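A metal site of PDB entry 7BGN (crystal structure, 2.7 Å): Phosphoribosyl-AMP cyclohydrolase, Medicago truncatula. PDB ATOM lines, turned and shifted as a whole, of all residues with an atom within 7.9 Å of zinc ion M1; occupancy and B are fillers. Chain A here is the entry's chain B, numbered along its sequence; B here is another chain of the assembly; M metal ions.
SG of Cys 97 lies close to OG1 of Thr 99, at 3.5 Å. The backbone NH (N) of Cys 104 is in hydrogen-bond range of the backbone carbonyl oxygen (O) of Leu 32 (3.1 Å).
Zinc ion M1 is bound by SG of Cys 81 of chain B (2.3 Å), SG of Cys 97 (2.3 Å) and SG of Cys 104 (2.5 Å).
Merely in contact with zinc ion M1: His 98 (3.6 Å). Four residues have an atom within 4 Å of zinc ion M1: Cys 97, His 98, Cys 104 and Cys 81 of chain B. The nearest printed residue that does not touch zinc ion M1 is Thr 99 (5.1 Å).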
ATOM      1  N   LEU A  32       3.439  -4.792 -17.086  1.00  0.00           N
ATOM      2  CA  LEU A  32       4.526  -5.719 -17.399  1.00  0.00           C
ATOM      3  C   LEU A  32       5.537  -5.815 -16.273  1.00  0.00           C
ATOM      4  O   LEU A  32       5.914  -6.914 -15.848  1.00  0.00           O
ATOM      5  CB  LEU A  32       5.223  -5.292 -18.691  1.00  0.00           C
ATOM      6  CG  LEU A  32       4.297  -5.151 -19.895  1.00  0.00           C
ATOM      7  CD1 LEU A  32       5.077  -4.765 -21.135  1.00  0.00           C
ATOM      8  CD2 LEU A  32       3.487  -6.429 -20.107  1.00  0.00           C
ATOM      9  N   MET A  33       5.982  -4.666 -15.764  1.00  0.00           N
ATOM     10  CA  MET A  33       7.060  -4.597 -14.789  1.00  0.00           C
ATOM     11  C   MET A  33       7.105  -3.184 -14.257  1.00  0.00           C
ATOM     12  O   MET A  33       6.557  -2.253 -14.858  1.00  0.00           O
ATOM     13  CB  MET A  33       8.411  -4.970 -15.415  1.00  0.00           C
ATOM     14  CG  MET A  33       8.780  -4.087 -16.611  1.00  0.00           C
ATOM     15  SD  MET A  33      10.547  -3.967 -16.980  1.00  0.00           S
ATOM     16  CE  MET A  33      11.161  -3.147 -15.508  1.00  0.00           C
ATOM     17  N   TRP A  62      19.818   0.448 -18.180  1.00  0.00           N
ATOM     18  CA  TRP A  62      19.388  -0.894 -18.564  1.00  0.00           C
ATOM     19  C   TRP A  62      18.137  -0.796 -19.420  1.00  0.00           C
ATOM     20  O   TRP A  62      17.098  -0.303 -18.957  1.00  0.00           O
ATOM     21  CB  TRP A  62      19.134  -1.752 -17.311  1.00  0.00           C
ATOM     22  CG  TRP A  62      18.224  -2.932 -17.553  1.00  0.00           C
ATOM     23  CD1 TRP A  62      18.421  -3.952 -18.446  1.00  0.00           C
ATOM     24  CD2 TRP A  62      17.001  -3.227 -16.873  1.00  0.00           C
ATOM     25  NE1 TRP A  62      17.379  -4.848 -18.369  1.00  0.00           N
ATOM     26  CE2 TRP A  62      16.492  -4.426 -17.415  1.00  0.00           C
ATOM     27  CE3 TRP A  62      16.277  -2.579 -15.867  1.00  0.00           C
ATOM     28  CZ2 TRP A  62      15.301  -5.001 -16.981  1.00  0.00           C
ATOM     29  CZ3 TRP A  62      15.099  -3.150 -15.443  1.00  0.00           C
ATOM     30  CH2 TRP A  62      14.617  -4.340 -15.995  1.00  0.00           C
ATOM     31  N   LYS A  64      15.187  -2.799 -21.019  1.00  0.00           N
ATOM     32  CA  LYS A  64      14.511  -4.087 -20.908  1.00  0.00           C
ATOM     33  C   LYS A  64      14.571  -4.825 -22.229  1.00  0.00           C
ATOM     34  O   LYS A  64      14.072  -4.326 -23.248  1.00  0.00           O
ATOM     35  CB  LYS A  64      13.066  -3.883 -20.470  1.00  0.00           C
ATOM     36  CG  LYS A  64      12.286  -5.167 -20.371  1.00  0.00           C
ATOM     37  CD  LYS A  64      13.049  -6.196 -19.570  1.00  0.00           C
ATOM     38  CE  LYS A  64      12.529  -7.586 -19.853  1.00  0.00           C
ATOM     39  NZ  LYS A  64      13.179  -8.637 -19.014  1.00  0.00           N
ATOM     40  N   THR A  96       7.910 -10.692 -20.270  1.00  0.00           N
ATOM     41  CA  THR A  96       8.683  -9.609 -19.686  1.00  0.00           C
ATOM     42  C   THR A  96       9.545 -10.092 -18.528  1.00  0.00           C
ATOM     43  O   THR A  96      10.726  -9.741 -18.452  1.00  0.00           O
ATOM     44  CB  THR A  96       7.760  -8.468 -19.244  1.00  0.00           C
ATOM     45  OG1 THR A  96       7.018  -7.990 -20.366  1.00  0.00           O
ATOM     46  CG2 THR A  96       8.578  -7.313 -18.656  1.00  0.00           C
ATOM     47  N   CYS A  97       9.006 -10.953 -17.663  1.00  0.00           N
ATOM     48  CA  CYS A  97       9.757 -11.378 -16.493  1.00  0.00           C
ATOM     49  C   CYS A  97      10.883 -12.329 -16.879  1.00  0.00           C
ATOM     50  O   CYS A  97      10.791 -13.078 -17.854  1.00  0.00           O
ATOM     51  CB  CYS A  97       8.858 -12.050 -15.461  1.00  0.00           C
ATOM     52  SG  CYS A  97       9.758 -12.585 -13.947  1.00  0.00           S
ATOM     53  N   HIS A  98      11.954 -12.294 -16.083  1.00  0.00           N
ATOM     54  CA  HIS A  98      13.129 -13.104 -16.370  1.00  0.00           C
ATOM     55  C   HIS A  98      12.887 -14.604 -16.158  1.00  0.00           C
ATOM     56  O   HIS A  98      13.648 -15.413 -16.678  1.00  0.00           O
ATOM     57  CB  HIS A  98      14.317 -12.604 -15.528  1.00  0.00           C
ATOM     58  CG  HIS A  98      14.472 -13.296 -14.211  1.00  0.00           C
ATOM     59  ND1 HIS A  98      13.741 -12.947 -13.091  1.00  0.00           N
ATOM     60  CD2 HIS A  98      15.314 -14.275 -13.806  1.00  0.00           C
ATOM     61  CE1 HIS A  98      14.108 -13.703 -12.069  1.00  0.00           C
ATOM     62  NE2 HIS A  98      15.061 -14.515 -12.484  1.00  0.00           N
ATOM     63  N   THR A  99      11.849 -14.978 -15.413  1.00  0.00           N
ATOM     64  CA  THR A  99      11.493 -16.382 -15.221  1.00  0.00           C
ATOM     65  C   THR A  99      10.785 -16.992 -16.421  1.00  0.00           C
ATOM     66  O   THR A  99      10.625 -18.217 -16.465  1.00  0.00           O
ATOM     67  CB  THR A  99      10.590 -16.567 -13.994  1.00  0.00           C
ATOM     68  OG1 THR A  99       9.300 -15.993 -14.256  1.00  0.00           O
ATOM     69  CG2 THR A  99      11.174 -15.871 -12.782  1.00  0.00           C
ATOM     70  N   GLY A 100      10.310 -16.180 -17.356  1.00  0.00           N
ATOM     71  CA  GLY A 100       9.528 -16.639 -18.474  1.00  0.00           C
ATOM     72  C   GLY A 100       8.065 -16.288 -18.378  1.00  0.00           C
ATOM     73  O   GLY A 100       7.330 -16.495 -19.359  1.00  0.00           O
ATOM     74  N   ALA A 101       7.614 -15.749 -17.257  1.00  0.00           N
ATOM     75  CA  ALA A 101       6.216 -15.366 -17.112  1.00  0.00           C
ATOM     76  C   ALA A 101       5.904 -14.192 -18.028  1.00  0.00           C
ATOM     77  O   ALA A 101       6.768 -13.366 -18.343  1.00  0.00           O
ATOM     78  CB  ALA A 101       5.903 -15.036 -15.658  1.00  0.00           C
ATOM     79  N   THR A 103       4.082 -11.501 -17.564  1.00  0.00           N
ATOM     80  CA  THR A 103       4.432 -10.326 -16.768  1.00  0.00           C
ATOM     81  C   THR A 103       5.160 -10.763 -15.513  1.00  0.00           C
ATOM     82  O   THR A 103       5.286 -11.955 -15.222  1.00  0.00           O
ATOM     83  CB  THR A 103       3.183  -9.500 -16.409  1.00  0.00           C
ATOM     84  OG1 THR A 103       2.403 -10.216 -15.446  1.00  0.00           O
ATOM     85  CG2 THR A 103       2.356  -9.270 -17.631  1.00  0.00           C
ATOM     86  N   CYS A 104       5.640  -9.788 -14.736  1.00  0.00           N
ATOM     87  CA  CYS A 104       6.371 -10.081 -13.515  1.00  0.00           C
ATOM     88  C   CYS A 104       5.468 -10.320 -12.324  1.00  0.00           C
ATOM     89  O   CYS A 104       5.945 -10.767 -11.271  1.00  0.00           O
ATOM     90  CB  CYS A 104       7.332  -8.935 -13.162  1.00  0.00           C
ATOM     91  SG  CYS A 104       8.886  -8.854 -14.067  1.00  0.00           S
ATOM     92  N   TYR A 105       4.174 -10.048 -12.439  1.00  0.00           N
ATOM     93  CA  TYR A 105       3.269 -10.067 -11.295  1.00  0.00           C
ATOM     94  C   TYR A 105       2.462 -11.352 -11.325  1.00  0.00           C
ATOM     95  O   TYR A 105       1.449 -11.440 -12.025  1.00  0.00           O
ATOM     96  CB  TYR A 105       2.405  -8.819 -11.313  1.00  0.00           C
ATOM     97  CG  TYR A 105       3.214  -7.543 -11.153  1.00  0.00           C
ATOM     98  CD1 TYR A 105       3.768  -6.905 -12.242  1.00  0.00           C
ATOM     99  CD2 TYR A 105       3.424  -6.996  -9.891  1.00  0.00           C
ATOM    100  CE1 TYR A 105       4.497  -5.746 -12.097  1.00  0.00           C
ATOM    101  CE2 TYR A 105       4.153  -5.834  -9.736  1.00  0.00           C
ATOM    102  CZ  TYR A 105       4.688  -5.223 -10.829  1.00  0.00           C
ATOM    103  OH  TYR A 105       5.407  -4.073 -10.650  1.00  0.00           O
ATOM    104  N   TYR A 106       2.897 -12.346 -10.548  1.00  0.00           N
ATOM    105  CA  TYR A 106       2.179 -13.618 -10.520  1.00  0.00           C
ATOM    106  C   TYR A 106       2.240 -14.270  -9.152  1.00  0.00           C
ATOM    107  O   TYR A 106       2.147 -15.491  -9.043  1.00  0.00           O
ATOM    108  CB  TYR A 106       2.748 -14.612 -11.551  1.00  0.00           C
ATOM    109  CG  TYR A 106       4.243 -14.744 -11.448  1.00  0.00           C
ATOM    110  CD1 TYR A 106       4.819 -15.609 -10.517  1.00  0.00           C
ATOM    111  CD2 TYR A 106       5.079 -14.003 -12.277  1.00  0.00           C
ATOM    112  CE1 TYR A 106       6.190 -15.725 -10.411  1.00  0.00           C
ATOM    113  CE2 TYR A 106       6.454 -14.113 -12.183  1.00  0.00           C
ATOM    114  CZ  TYR A 106       6.998 -14.973 -11.246  1.00  0.00           C
ATOM    115  OH  TYR A 106       8.370 -15.092 -11.150  1.00  0.00           O
ATOM    116  N   ASP B  80       5.532  -8.794  -7.256  1.00  0.00           N
ATOM    117  CA  ASP B  80       6.314  -9.207  -8.413  1.00  0.00           C
ATOM    118  C   ASP B  80       7.369 -10.241  -7.980  1.00  0.00           C
ATOM    119  O   ASP B  80       7.406 -10.689  -6.836  1.00  0.00           O
ATOM    120  CB  ASP B  80       6.940  -7.993  -9.117  1.00  0.00           C
ATOM    121  CG  ASP B  80       7.942  -7.274  -8.269  1.00  0.00           C
ATOM    122  OD1 ASP B  80       7.799  -7.282  -7.038  1.00  0.00           O
ATOM    123  OD2 ASP B  80       8.892  -6.674  -8.841  1.00  0.00           O
ATOM    124  N   CYS B  81       8.215 -10.626  -8.940  1.00  0.00           N
ATOM    125  CA  CYS B  81       9.141 -11.738  -8.738  1.00  0.00           C
ATOM    126  C   CYS B  81      10.146 -11.478  -7.619  1.00  0.00           C
ATOM    127  O   CYS B  81      10.375 -12.337  -6.768  1.00  0.00           O
ATOM    128  CB  CYS B  81       9.840 -12.050 -10.052  1.00  0.00           C
ATOM    129  SG  CYS B  81      10.329 -10.588 -10.984  1.00  0.00           S
ATOM    130  N   ASP B  82      10.785 -10.305  -7.635  1.00  0.00           N
ATOM    131  CA  ASP B  82      11.734  -9.912  -6.595  1.00  0.00           C
ATOM    132  C   ASP B  82      11.036  -9.400  -5.322  1.00  0.00           C
ATOM    133  O   ASP B  82      11.725  -9.108  -4.341  1.00  0.00           O
ATOM    134  CB  ASP B  82      12.686  -8.839  -7.136  1.00  0.00           C
ATOM    135  CG  ASP B  82      11.961  -7.735  -7.894  1.00  0.00           C
ATOM    136  OD1 ASP B  82      10.708  -7.772  -7.940  1.00  0.00           O
ATOM    137  OD2 ASP B  82      12.627  -6.836  -8.432  1.00  0.00           O
HETATM  138 ZN    ZN M   1      10.547 -10.507 -13.271  1.00  0.00          ZN
HETATM  139 ZN    ZN M   2      10.787  -5.905  -8.673  1.00  0.00          ZN
